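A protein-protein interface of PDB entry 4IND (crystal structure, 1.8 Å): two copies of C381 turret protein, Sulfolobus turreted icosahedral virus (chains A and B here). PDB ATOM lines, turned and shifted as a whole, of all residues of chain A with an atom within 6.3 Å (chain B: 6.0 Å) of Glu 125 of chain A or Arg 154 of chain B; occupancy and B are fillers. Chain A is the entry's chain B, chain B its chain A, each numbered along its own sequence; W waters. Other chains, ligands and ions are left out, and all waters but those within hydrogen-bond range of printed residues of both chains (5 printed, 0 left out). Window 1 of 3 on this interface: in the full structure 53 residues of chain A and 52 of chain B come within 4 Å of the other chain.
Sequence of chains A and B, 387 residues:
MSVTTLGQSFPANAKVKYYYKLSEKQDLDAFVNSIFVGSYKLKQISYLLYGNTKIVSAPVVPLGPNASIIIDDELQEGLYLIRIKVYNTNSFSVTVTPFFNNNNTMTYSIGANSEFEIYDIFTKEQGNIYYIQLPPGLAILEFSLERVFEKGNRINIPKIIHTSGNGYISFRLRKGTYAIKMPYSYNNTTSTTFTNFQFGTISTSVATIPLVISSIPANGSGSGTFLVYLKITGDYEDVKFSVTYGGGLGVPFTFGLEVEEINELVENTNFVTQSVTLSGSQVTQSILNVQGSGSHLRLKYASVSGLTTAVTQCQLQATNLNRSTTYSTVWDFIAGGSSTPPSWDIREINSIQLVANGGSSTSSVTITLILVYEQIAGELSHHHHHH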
ATOM      1  N   GLU A  77       0.543   9.461 -20.009  1.00  0.00           N
ATOM      2  CA  GLU A  77      -0.438   9.010 -19.017  1.00  0.00           C
ATOM      3  C   GLU A  77       0.267   8.598 -17.734  1.00  0.00           C
ATOM      4  O   GLU A  77       1.427   8.198 -17.759  1.00  0.00           O
ATOM      5  CB  GLU A  77      -1.279   7.857 -19.574  1.00  0.00           C
ATOM      6  CG  GLU A  77      -2.243   8.325 -20.667  1.00  0.00           C
ATOM      7  CD  GLU A  77      -3.338   7.309 -20.980  1.00  0.00           C
ATOM      8  OE1 GLU A  77      -3.056   6.088 -20.910  1.00  0.00           O
ATOM      9  OE2 GLU A  77      -4.476   7.743 -21.297  1.00  0.00           O
ATOM     10  N   GLY A  78      -0.429   8.710 -16.604  1.00  0.00           N
ATOM     11  CA  GLY A  78       0.150   8.315 -15.331  1.00  0.00           C
ATOM     12  C   GLY A  78      -0.372   9.173 -14.202  1.00  0.00           C
ATOM     13  O   GLY A  78      -1.238  10.033 -14.402  1.00  0.00           O
ATOM     14  N   PHE A 122      -2.834  14.693  -9.913  1.00  0.00           N
ATOM     15  CA  PHE A 122      -3.545  14.681 -11.185  1.00  0.00           C
ATOM     16  C   PHE A 122      -3.327  13.349 -11.855  1.00  0.00           C
ATOM     17  O   PHE A 122      -2.191  12.975 -12.149  1.00  0.00           O
ATOM     18  CB  PHE A 122      -2.977  15.791 -12.076  1.00  0.00           C
ATOM     19  CG  PHE A 122      -3.560  15.833 -13.470  1.00  0.00           C
ATOM     20  CD1 PHE A 122      -4.935  15.767 -13.674  1.00  0.00           C
ATOM     21  CD2 PHE A 122      -2.728  15.989 -14.576  1.00  0.00           C
ATOM     22  CE1 PHE A 122      -5.470  15.844 -14.987  1.00  0.00           C
ATOM     23  CE2 PHE A 122      -3.255  16.088 -15.872  1.00  0.00           C
ATOM     24  CZ  PHE A 122      -4.609  15.998 -16.077  1.00  0.00           C
ATOM     25  N   THR A 123      -4.405  12.620 -12.104  1.00  0.00           N
ATOM     26  CA  THR A 123      -4.298  11.371 -12.862  1.00  0.00           C
ATOM     27  C   THR A 123      -4.567  11.632 -14.327  1.00  0.00           C
ATOM     28  O   THR A 123      -5.697  11.971 -14.701  1.00  0.00           O
ATOM     29  CB  THR A 123      -5.331  10.353 -12.386  1.00  0.00           C
ATOM     30  OG1 THR A 123      -5.150  10.097 -10.979  1.00  0.00           O
ATOM     31  CG2 THR A 123      -5.187   9.038 -13.185  1.00  0.00           C
ATOM     32  N   LYS A 124      -3.537  11.493 -15.167  1.00  0.00           N
ATOM     33  CA  LYS A 124      -3.720  11.644 -16.613  1.00  0.00           C
ATOM     34  C   LYS A 124      -4.152  10.301 -17.198  1.00  0.00           C
ATOM     35  O   LYS A 124      -3.320   9.465 -17.533  1.00  0.00           O
ATOM     36  CB  LYS A 124      -2.435  12.145 -17.322  1.00  0.00           C
ATOM     37  CG  LYS A 124      -2.660  12.406 -18.812  1.00  0.00           C
ATOM     38  CD  LYS A 124      -3.698  13.521 -18.965  1.00  0.00           C
ATOM     39  CE  LYS A 124      -4.268  13.631 -20.383  1.00  0.00           C
ATOM     40  NZ  LYS A 124      -5.286  14.712 -20.435  1.00  0.00           N
ATOM     41  N   GLU A 125      -5.461  10.103 -17.282  1.00  0.00           N
ATOM     42  CA  GLU A 125      -6.077   8.963 -17.954  1.00  0.00           C
ATOM     43  C   GLU A 125      -7.442   9.440 -18.442  1.00  0.00           C
ATOM     44  O   GLU A 125      -8.009  10.384 -17.880  1.00  0.00           O
ATOM     45  CB  GLU A 125      -6.282   7.793 -16.982  1.00  0.00           C
ATOM     46  CG  GLU A 125      -5.061   6.917 -16.767  1.00  0.00           C
ATOM     47  CD  GLU A 125      -5.382   5.614 -16.025  1.00  0.00           C
ATOM     48  OE1 GLU A 125      -6.419   5.561 -15.326  1.00  0.00           O
ATOM     49  OE2 GLU A 125      -4.591   4.650 -16.140  1.00  0.00           O
ATOM     50  N   GLN A 126      -7.963   8.789 -19.476  1.00  0.00           N
ATOM     51  CA  GLN A 126      -9.304   9.090 -19.984  1.00  0.00           C
ATOM     52  C   GLN A 126      -9.593  10.590 -20.173  1.00  0.00           C
ATOM     53  O   GLN A 126     -10.673  11.069 -19.817  1.00  0.00           O
ATOM     54  CB  GLN A 126     -10.361   8.479 -19.065  1.00  0.00           C
ATOM     55  CG  GLN A 126     -10.322   6.952 -18.983  1.00  0.00           C
ATOM     56  CD  GLN A 126     -11.610   6.376 -18.411  1.00  0.00           C
ATOM     57  OE1 GLN A 126     -12.463   7.116 -17.930  1.00  0.00           O
ATOM     58  NE2 GLN A 126     -11.760   5.057 -18.473  1.00  0.00           N
ATOM     59  N   GLY A 127      -8.642  11.329 -20.730  1.00  0.00           N
ATOM     60  CA  GLY A 127      -8.870  12.739 -21.027  1.00  0.00           C
ATOM     61  C   GLY A 127      -9.091  13.676 -19.850  1.00  0.00           C
ATOM     62  O   GLY A 127      -9.608  14.782 -20.028  1.00  0.00           O
ATOM     63  N   ASN A 128      -8.707  13.246 -18.651  1.00  0.00           N
ATOM     64  CA  ASN A 128      -8.838  14.078 -17.449  1.00  0.00           C
ATOM     65  C   ASN A 128      -8.165  15.429 -17.654  1.00  0.00           C
ATOM     66  O   ASN A 128      -7.109  15.517 -18.285  1.00  0.00           O
ATOM     67  CB  ASN A 128      -8.191  13.366 -16.257  1.00  0.00           C
ATOM     68  CG  ASN A 128      -8.627  13.945 -14.912  1.00  0.00           C
ATOM     69  OD1 ASN A 128      -9.603  14.693 -14.827  1.00  0.00           O
ATOM     70  ND2 ASN A 128      -7.909  13.583 -13.851  1.00  0.00           N
ATOM     71  N   ILE A 129      -8.750  16.484 -17.096  1.00  0.00           N
ATOM     72  CA  ILE A 129      -8.250  17.838 -17.327  1.00  0.00           C
ATOM     73  C   ILE A 129      -7.876  18.495 -16.012  1.00  0.00           C
ATOM     74  O   ILE A 129      -8.717  18.618 -15.124  1.00  0.00           O
ATOM     75  CB  ILE A 129      -9.329  18.706 -17.984  1.00  0.00           C
ATOM     76  CG1 ILE A 129      -9.767  18.084 -19.309  1.00  0.00           C
ATOM     77  CG2 ILE A 129      -8.837  20.153 -18.119  1.00  0.00           C
ATOM     78  CD1 ILE A 129     -11.112  18.566 -19.799  1.00  0.00           C
ATOM     79  N   ARG A 172      -4.631   6.974  -9.055  1.00  0.00           N
ATOM     80  CA  ARG A 172      -4.565   5.646  -9.659  1.00  0.00           C
ATOM     81  C   ARG A 172      -3.305   5.002  -9.134  1.00  0.00           C
ATOM     82  O   ARG A 172      -2.255   5.631  -9.155  1.00  0.00           O
ATOM     83  CB  ARG A 172      -4.444   5.745 -11.184  1.00  0.00           C
ATOM     84  CG  ARG A 172      -4.256   4.370 -11.851  1.00  0.00           C
ATOM     85  CD  ARG A 172      -3.481   4.421 -13.153  1.00  0.00           C
ATOM     86  NE  ARG A 172      -2.047   4.637 -12.952  1.00  0.00           N
ATOM     87  CZ  ARG A 172      -1.176   4.730 -13.960  1.00  0.00           C
ATOM     88  NH1 ARG A 172      -1.598   4.630 -15.213  1.00  0.00           N
ATOM     89  NH2 ARG A 172       0.114   4.925 -13.726  1.00  0.00           N
ATOM     90  N   GLY A 234      -4.256  -5.054  -9.174  1.00  0.00           N
ATOM     91  CA  GLY A 234      -4.031  -4.417 -10.457  1.00  0.00           C
ATOM     92  C   GLY A 234      -5.268  -4.332 -11.323  1.00  0.00           C
ATOM     93  O   GLY A 234      -5.263  -3.606 -12.312  1.00  0.00           O
ATOM     94  N   ASP A 235      -6.312  -5.084 -10.987  1.00  0.00           N
ATOM     95  CA  ASP A 235      -7.537  -5.000 -11.773  1.00  0.00           C
ATOM     96  C   ASP A 235      -8.459  -3.862 -11.319  1.00  0.00           C
ATOM     97  O   ASP A 235      -9.392  -3.507 -12.035  1.00  0.00           O
ATOM     98  CB  ASP A 235      -8.281  -6.353 -11.873  1.00  0.00           C
ATOM     99  CG  ASP A 235      -8.493  -7.040 -10.505  1.00  0.00           C
ATOM    100  OD1 ASP A 235      -7.897  -6.632  -9.489  1.00  0.00           O
ATOM    101  OD2 ASP A 235      -9.234  -8.029 -10.471  1.00  0.00           O
ATOM    102  N   TYR A 236      -8.172  -3.280 -10.156  1.00  0.00           N
ATOM    103  CA  TYR A 236      -8.889  -2.093  -9.668  1.00  0.00           C
ATOM    104  C   TYR A 236      -7.868  -1.113  -9.154  1.00  0.00           C
ATOM    105  O   TYR A 236      -7.316  -1.291  -8.084  1.00  0.00           O
ATOM    106  CB  TYR A 236      -9.912  -2.477  -8.566  1.00  0.00           C
ATOM    107  CG  TYR A 236     -11.028  -3.304  -9.116  1.00  0.00           C
ATOM    108  CD1 TYR A 236     -12.183  -2.714  -9.598  1.00  0.00           C
ATOM    109  CD2 TYR A 236     -10.924  -4.675  -9.179  1.00  0.00           C
ATOM    110  CE1 TYR A 236     -13.188  -3.461 -10.135  1.00  0.00           C
ATOM    111  CE2 TYR A 236     -11.939  -5.439  -9.711  1.00  0.00           C
ATOM    112  CZ  TYR A 236     -13.067  -4.826 -10.187  1.00  0.00           C
ATOM    113  OH  TYR A 236     -14.082  -5.578 -10.717  1.00  0.00           O
ATOM    114  N   GLU A 237      -7.594  -0.062  -9.927  1.00  0.00           N
ATOM    115  CA  GLU A 237      -6.460   0.802  -9.629  1.00  0.00           C
ATOM    116  C   GLU A 237      -6.864   2.164  -9.107  1.00  0.00           C
ATOM    117  O   GLU A 237      -6.066   2.858  -8.497  1.00  0.00           O
ATOM    118  CB  GLU A 237      -5.560   0.927 -10.905  1.00  0.00           C
ATOM    119  CG  GLU A 237      -5.071  -0.440 -11.387  1.00  0.00           C
ATOM    120  CD  GLU A 237      -4.004  -0.369 -12.483  1.00  0.00           C
ATOM    121  OE1 GLU A 237      -3.554   0.749 -12.826  1.00  0.00           O
ATOM    122  OE2 GLU A 237      -3.647  -1.443 -13.027  1.00  0.00           O
ATOM    123  N   ASP A 238      -8.104   2.561  -9.351  1.00  0.00           N
ATOM    124  CA  ASP A 238      -8.524   3.895  -8.940  1.00  0.00           C
ATOM    125  C   ASP A 238      -8.937   3.916  -7.467  1.00  0.00           C
ATOM    126  O   ASP A 238      -9.829   3.191  -7.050  1.00  0.00           O
ATOM    127  CB  ASP A 238      -9.619   4.428  -9.878  1.00  0.00           C
ATOM    128  CG  ASP A 238      -9.050   4.864 -11.247  1.00  0.00           C
ATOM    129  OD1 ASP A 238      -8.242   5.816 -11.299  1.00  0.00           O
ATOM    130  OD2 ASP A 238      -9.395   4.246 -12.272  1.00  0.00           O
ATOM    131  N   LEU B  81      -0.190   3.253 -27.322  1.00  0.00           N
ATOM    132  CA  LEU B  81      -1.481   3.868 -27.159  1.00  0.00           C
ATOM    133  C   LEU B  81      -1.383   5.181 -27.900  1.00  0.00           C
ATOM    134  O   LEU B  81      -0.487   5.995 -27.632  1.00  0.00           O
ATOM    135  CB  LEU B  81      -1.778   4.153 -25.682  1.00  0.00           C
ATOM    136  CG  LEU B  81      -3.043   5.009 -25.522  1.00  0.00           C
ATOM    137  CD1 LEU B  81      -4.269   4.113 -25.639  1.00  0.00           C
ATOM    138  CD2 LEU B  81      -3.047   5.812 -24.210  1.00  0.00           C
ATOM    139  N   TYR B 119      -8.908   7.470 -29.073  1.00  0.00           N
ATOM    140  CA  TYR B 119      -7.896   6.542 -28.570  1.00  0.00           C
ATOM    141  C   TYR B 119      -7.673   5.475 -29.613  1.00  0.00           C
ATOM    142  O   TYR B 119      -8.624   5.004 -30.242  1.00  0.00           O
ATOM    143  CB  TYR B 119      -8.360   5.865 -27.264  1.00  0.00           C
ATOM    144  CG  TYR B 119      -8.609   6.832 -26.144  1.00  0.00           C
ATOM    145  CD1 TYR B 119      -7.658   7.048 -25.148  1.00  0.00           C
ATOM    146  CD2 TYR B 119      -9.792   7.538 -26.082  1.00  0.00           C
ATOM    147  CE1 TYR B 119      -7.898   7.953 -24.111  1.00  0.00           C
ATOM    148  CE2 TYR B 119     -10.034   8.425 -25.061  1.00  0.00           C
ATOM    149  CZ  TYR B 119      -9.086   8.640 -24.086  1.00  0.00           C
ATOM    150  OH  TYR B 119      -9.369   9.554 -23.082  1.00  0.00           O
ATOM    151  N   GLU B 146       2.458   6.812 -27.370  1.00  0.00           N
ATOM    152  CA  GLU B 146       3.212   6.450 -26.162  1.00  0.00           C
ATOM    153  C   GLU B 146       3.143   4.947 -25.964  1.00  0.00           C
ATOM    154  O   GLU B 146       2.116   4.332 -26.215  1.00  0.00           O
ATOM    155  CB  GLU B 146       2.690   7.204 -24.916  1.00  0.00           C
ATOM    156  CG  GLU B 146       1.379   6.658 -24.361  1.00  0.00           C
ATOM    157  CD  GLU B 146       1.207   6.883 -22.843  1.00  0.00           C
ATOM    158  OE1 GLU B 146       1.291   8.048 -22.377  1.00  0.00           O
ATOM    159  OE2 GLU B 146       0.956   5.884 -22.124  1.00  0.00           O
ATOM    160  N   VAL B 148       2.647   1.744 -23.846  1.00  0.00           N
ATOM    161  CA  VAL B 148       1.955   1.418 -22.582  1.00  0.00           C
ATOM    162  C   VAL B 148       2.683   0.278 -21.877  1.00  0.00           C
ATOM    163  O   VAL B 148       3.460  -0.424 -22.489  1.00  0.00           O
ATOM    164  CB  VAL B 148       0.498   1.029 -22.851  1.00  0.00           C
ATOM    165  CG1 VAL B 148      -0.232   2.175 -23.506  1.00  0.00           C
ATOM    166  CG2 VAL B 148       0.426  -0.184 -23.758  1.00  0.00           C
ATOM    167  N   PHE B 149       2.457   0.081 -20.592  1.00  0.00           N
ATOM    168  CA  PHE B 149       3.168  -0.981 -19.901  1.00  0.00           C
ATOM    169  C   PHE B 149       4.616  -0.553 -19.710  1.00  0.00           C
ATOM    170  O   PHE B 149       5.486  -1.366 -19.408  1.00  0.00           O
ATOM    171  CB  PHE B 149       3.063  -2.300 -20.686  1.00  0.00           C
ATOM    172  CG  PHE B 149       1.640  -2.720 -20.953  1.00  0.00           C
ATOM    173  CD1 PHE B 149       0.705  -2.749 -19.911  1.00  0.00           C
ATOM    174  CD2 PHE B 149       1.220  -3.038 -22.230  1.00  0.00           C
ATOM    175  CE1 PHE B 149      -0.618  -3.095 -20.156  1.00  0.00           C
ATOM    176  CE2 PHE B 149      -0.104  -3.404 -22.478  1.00  0.00           C
ATOM    177  CZ  PHE B 149      -1.019  -3.430 -21.430  1.00  0.00           C
ATOM    178  N   GLY B 152       4.471   1.432 -15.604  1.00  0.00           N
ATOM    179  CA  GLY B 152       3.284   0.967 -14.924  1.00  0.00           C
ATOM    180  C   GLY B 152       2.008   1.527 -15.499  1.00  0.00           C
ATOM    181  O   GLY B 152       0.977   1.504 -14.829  1.00  0.00           O
ATOM    182  N   ASN B 153       2.057   2.023 -16.734  1.00  0.00           N
ATOM    183  CA  ASN B 153       0.823   2.459 -17.382  1.00  0.00           C
ATOM    184  C   ASN B 153      -0.006   1.301 -17.902  1.00  0.00           C
ATOM    185  O   ASN B 153       0.477   0.185 -18.030  1.00  0.00           O
ATOM    186  CB  ASN B 153       1.100   3.479 -18.484  1.00  0.00           C
ATOM    187  CG  ASN B 153       1.427   4.843 -17.917  1.00  0.00           C
ATOM    188  OD1 ASN B 153       1.037   5.164 -16.787  1.00  0.00           O
ATOM    189  ND2 ASN B 153       2.157   5.648 -18.680  1.00  0.00           N
ATOM    190  N   ARG B 154      -1.268   1.579 -18.184  1.00  0.00           N
ATOM    191  CA  ARG B 154      -2.170   0.578 -18.696  1.00  0.00           C
ATOM    192  C   ARG B 154      -2.905   1.179 -19.865  1.00  0.00           C
ATOM    193  O   ARG B 154      -2.901   2.399 -20.054  1.00  0.00           O
ATOM    194  CB  ARG B 154      -3.201   0.207 -17.623  1.00  0.00           C
ATOM    195  CG  ARG B 154      -3.920   1.427 -17.051  1.00  0.00           C
ATOM    196  CD  ARG B 154      -5.081   1.023 -16.134  1.00  0.00           C
ATOM    197  NE  ARG B 154      -5.670   2.194 -15.475  1.00  0.00           N
ATOM    198  CZ  ARG B 154      -6.627   2.120 -14.552  1.00  0.00           C
ATOM    199  NH1 ARG B 154      -7.082   0.941 -14.186  1.00  0.00           N
ATOM    200  NH2 ARG B 154      -7.130   3.214 -14.005  1.00  0.00           N
ATOM    201  N   ILE B 155      -3.533   0.325 -20.650  1.00  0.00           N
ATOM    202  CA  ILE B 155      -4.508   0.785 -21.629  1.00  0.00           C
ATOM    203  C   ILE B 155      -5.782   1.074 -20.843  1.00  0.00           C
ATOM    204  O   ILE B 155      -6.249   0.226 -20.081  1.00  0.00           O
ATOM    205  CB  ILE B 155      -4.791  -0.306 -22.667  1.00  0.00           C
ATOM    206  CG1 ILE B 155      -3.543  -0.542 -23.532  1.00  0.00           C
ATOM    207  CG2 ILE B 155      -5.973   0.082 -23.569  1.00  0.00           C
ATOM    208  CD1 ILE B 155      -3.697  -1.731 -24.470  1.00  0.00           C
ATOM    209  N   ASN B 156      -6.313   2.286 -20.993  1.00  0.00           N
ATOM    210  CA  ASN B 156      -7.565   2.662 -20.317  1.00  0.00           C
ATOM    211  C   ASN B 156      -8.410   3.546 -21.255  1.00  0.00           C
ATOM    212  O   ASN B 156      -8.369   4.759 -21.190  1.00  0.00           O
ATOM    213  CB  ASN B 156      -7.277   3.357 -18.996  1.00  0.00           C
ATOM    214  CG  ASN B 156      -8.543   3.605 -18.179  1.00  0.00           C
ATOM    215  OD1 ASN B 156      -9.626   3.182 -18.576  1.00  0.00           O
ATOM    216  ND2 ASN B 156      -8.408   4.295 -17.042  1.00  0.00           N
ATOM    217  N   LYS B 181     -10.458  -5.633 -18.863  1.00  0.00           N
ATOM    218  CA  LYS B 181     -11.746  -5.218 -18.350  1.00  0.00           C
ATOM    219  C   LYS B 181     -12.468  -4.443 -19.446  1.00  0.00           C
ATOM    220  O   LYS B 181     -11.899  -3.535 -20.076  1.00  0.00           O
ATOM    221  CB  LYS B 181     -11.582  -4.356 -17.087  1.00  0.00           C
ATOM    222  CG  LYS B 181     -12.903  -4.004 -16.402  1.00  0.00           C
ATOM    223  CD  LYS B 181     -12.710  -2.981 -15.279  1.00  0.00           C
ATOM    224  CE  LYS B 181     -11.819  -3.531 -14.159  1.00  0.00           C
ATOM    225  NZ  LYS B 181     -11.733  -2.554 -13.019  1.00  0.00           N
ATOM    226  N   GLU B 258      -9.830  -1.759 -20.932  1.00  0.00           N
ATOM    227  CA  GLU B 258      -8.793  -1.533 -19.942  1.00  0.00           C
ATOM    228  C   GLU B 258      -7.953  -2.806 -19.941  1.00  0.00           C
ATOM    229  O   GLU B 258      -8.470  -3.918 -19.768  1.00  0.00           O
ATOM    230  CB  GLU B 258      -9.493  -1.241 -18.598  1.00  0.00           C
ATOM    231  CG  GLU B 258      -8.633  -0.978 -17.373  1.00  0.00           C
ATOM    232  CD  GLU B 258      -9.509  -0.662 -16.149  1.00  0.00           C
ATOM    233  OE1 GLU B 258     -10.264   0.336 -16.221  1.00  0.00           O
ATOM    234  OE2 GLU B 258      -9.465  -1.420 -15.136  1.00  0.00           O
ATOM    235  N   VAL B 259      -6.654  -2.658 -20.194  1.00  0.00           N
ATOM    236  CA  VAL B 259      -5.720  -3.786 -20.139  1.00  0.00           C
ATOM    237  C   VAL B 259      -4.592  -3.399 -19.213  1.00  0.00           C
ATOM    238  O   VAL B 259      -3.926  -2.393 -19.444  1.00  0.00           O
ATOM    239  CB  VAL B 259      -5.123  -4.084 -21.532  1.00  0.00           C
ATOM    240  CG1 VAL B 259      -4.262  -5.352 -21.483  1.00  0.00           C
ATOM    241  CG2 VAL B 259      -6.229  -4.213 -22.567  1.00  0.00           C
ATOM    242  N   GLU B 260      -4.371  -4.185 -18.168  1.00  0.00           N
ATOM    243  CA  GLU B 260      -3.443  -3.796 -17.116  1.00  0.00           C
ATOM    244  C   GLU B 260      -2.769  -5.012 -16.516  1.00  0.00           C
ATOM    245  O   GLU B 260      -3.388  -6.079 -16.381  1.00  0.00           O
ATOM    246  CB  GLU B 260      -4.201  -3.029 -16.023  1.00  0.00           C
ATOM    247  CG  GLU B 260      -5.380  -3.810 -15.499  1.00  0.00           C
ATOM    248  CD  GLU B 260      -6.536  -2.933 -15.044  1.00  0.00           C
ATOM    249  OE1 GLU B 260      -6.347  -1.710 -14.856  1.00  0.00           O
ATOM    250  OE2 GLU B 260      -7.647  -3.472 -14.871  1.00  0.00           O
ATOM    251  N   GLU B 261      -1.495  -4.869 -16.158  1.00  0.00           N
ATOM    252  CA  GLU B 261      -0.765  -5.963 -15.536  1.00  0.00           C
ATOM    253  C   GLU B 261      -1.204  -6.127 -14.079  1.00  0.00           C
ATOM    254  O   GLU B 261      -1.434  -5.137 -13.374  1.00  0.00           O
ATOM    255  CB  GLU B 261       0.744  -5.702 -15.603  1.00  0.00           C
ATOM    256  CG  GLU B 261       1.589  -6.942 -15.346  1.00  0.00           C
ATOM    257  CD  GLU B 261       3.090  -6.682 -15.437  1.00  0.00           C
ATOM    258  OE1 GLU B 261       3.494  -5.575 -15.866  1.00  0.00           O
ATOM    259  OE2 GLU B 261       3.862  -7.586 -15.069  1.00  0.00           O
HETATM  260  O   HOH W   1     -11.647  11.002 -23.128  1.00  0.00           O
HETATM  261  O   HOH W   2      -7.073  11.158 -23.694  1.00  0.00           O
HETATM  262  O   HOH W   3      -0.606  -2.595 -12.789  1.00  0.00           O
HETATM  263  O   HOH W   4      -2.097   4.552 -17.587  1.00  0.00           O
HETATM  264  O   HOH W   5      -6.583   6.679 -20.319  1.00  0.00           O
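NE2 of Gln 126 of chain A lies within hydrogen-bond range of OD1 of Asn 156 of chain B (2.8 Å). O of Gly 234 of chain A sits close to OE1 of Glu 260 of chain B (3.4 Å). The side-chain carboxylate of Asp 238 of chain A is in salt-bridge range of the guanidinium group of Arg 154 of chain B, 3.0 Å away. The side-chain hydroxyl (OH) of Tyr 119 of chain B lies within hydrogen-bond range of the backbone NH (N) of Gly 127 of chain A. The side-chain amino group of Lys 181 of chain B is in hydrogen-bond range of the backbone carbonyl oxygen of Asp 235 of chain A (2.7 Å). The guanidinium group (NE) of Arg 154 of chain B lies within salt-bridge range of the side-chain carboxylate (OE2) of Glu 125 of chain A (2.8 Å). The side-chain carboxylate of Glu 260 of chain B lies close to the side-chain carboxylate of Glu 237 of chain A (3.3 Å). OD1 of Asn 153 of chain B lies within hydrogen-bond range of NH1 of Arg 172 of chain A, at 3.1 Å. O of Asp 235 of chain A sits close to OE2 of Glu 260 of chain B (3.3 Å). ND2 of Asn 153 of chain B lies within hydrogen-bond range of O of Glu 77 of chain A. The backbone NH of Glu 77 of chain A lies within hydrogen-bond range of the side-chain carboxylate of Glu 146 of chain B, at 2.9 Å. The side-chain amide nitrogen (ND2) of Asn 156 of chain B is in hydrogen-bond range of the side-chain carboxylate (OE1) of Glu 125 of chain A, at 2.9 Å. The guanidinium group of Arg 154 of chain B is in salt-bridge range of the side-chain carboxylate of Glu 237 of chain A, 3.7 Å away.
The backbone carbonyl oxygen of Gly 78 of chain A sits at hydrogen-bond distance from the backbone NH of Lys 124 of chain A, at 2.8 Å. OE2 of Glu 258 of chain B lies within salt-bridge range of NZ of Lys 181 of chain B, at 3.3 Å. The guanidinium group (NH1) of Arg 154 of chain B is in salt-bridge range of the side-chain carboxylate (OE2) of Glu 258 of chain B (3.5 Å). The backbone carbonyl oxygen of Glu 146 of chain B lies within hydrogen-bond range of the backbone NH of Leu 81 of chain B (2.8 Å). NH2 of Arg 154 of chain B sits close to ND2 of Asn 156 of chain B, at 3.5 Å. The guanidinium group (NH1) of Arg 154 of chain B lies within salt-bridge range of the side-chain carboxylate (OE1) of Glu 260 of chain B, 2.8 Å away.
Among the printed residues, pairs that only touch across the chains: Glu 77 of chain A with Leu 81 of chain B (3.3 Å), Glu 77 of chain A with Arg 154 of chain B (3.8 Å), Gly 78 of chain A with Asn 153 of chain B (3.6 Å), Gln 126 of chain A with Tyr 119 of chain B (3.1 Å), Arg 172 of chain A with Gly 152 of chain B (3.7 Å), Arg 172 of chain A with Arg 154 of chain B (3.8 Å), Gly 234 of chain A with Glu 261 of chain B (3.97 Å), Asp 235 of chain A with Glu 258 of chain B (3.7 Å) and Tyr 236 of chain A with Lys 181 of chain B (3.4 Å).
Glu 125 of chain A touches just these residues of chain B: Arg 154 (2.8 Å) and Asn 156 (2.9 Å). Ile 129 of chain A touches none of the printed residues of chain B. Printed residues of chain B within 4 Å of Asp 235 of chain A: Lys 181, Glu 258 and Glu 260. Of the printed residues of chain A, Glu 146 of chain B touches Glu 77 (2.9 Å). Arg 154 of chain B touches just these residues of chain A: Glu 77, Glu 125, Arg 172, Glu 237 and Asp 238. Of the printed residues of chain A, Glu 260 of chain B touches Gly 234 (3.1 Å), Asp 235 (3.3 Å) and Glu 237 (3.3 Å). The nearest residue of chain B that does not touch Glu 125 of chain A is Tyr 119 of chain B (5.0 Å). The nearest printed residue of chain B that does not touch Arg 172 of chain A is Asn 156 of chain B (6.3 Å).
Of the 15 printed residues of chain B, 11 touch a printed residue of chain A. Printed residues of chain B that touch a printed residue of chain A: Leu 81, Tyr 119, Glu 146, Gly 152, Asn 153, Arg 154, Asn 156, Lys 181, Glu 258, Glu 260 and Glu 261. Hydrophobic or aromatic side chains of chain B within 4 Å of the printed part of chain A: Leu 81 and Tyr 119. Hydrophobic or aromatic side chains of chain A within 4 Å of the printed part of chain B: Tyr 236. Among the printed residues, Asp or Glu carboxylates within 4 Å of a Lys or Arg side-chain nitrogen of the other chain: Glu 125 of chain A with Arg 154 of chain B, Glu 237 of chain A with Arg 154 of chain B and Asp 238 of chain A with Arg 154 of chain B.
No position is printed for both chains. Of the 22 pairs that touch across the chains among the printed residues, none has its exchanged pair printed and touching as well.
Water W4 lies within hydrogen-bond range of the guanidinium group of Arg 172 of chain A, the side-chain carboxylate of Glu 125 of chain A, the backbone NH of Arg 154 of chain B and the side-chain amide oxygen of Asn 153 of chain B. Water W5 lies within hydrogen-bond range of OE2 of Glu 77 of chain A (2.6 Å), N of Gln 126 of chain A (2.7 Å) and O of Asn 156 of chain B (2.8 Å). Water W1 bridges the side-chain hydroxyl (OH) of Tyr 119 of chain B (2.7 Å) and the backbone carbonyl oxygen (O) of Gln 126 of chain A (3.5 Å). Water W3 lies within hydrogen-bond range of O of Glu 261 of chain B and OE2 of Glu 237 of chain A. Water W2 lies within hydrogen-bond range of OH of Tyr 119 of chain B and N of Gly 127 of chain A.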
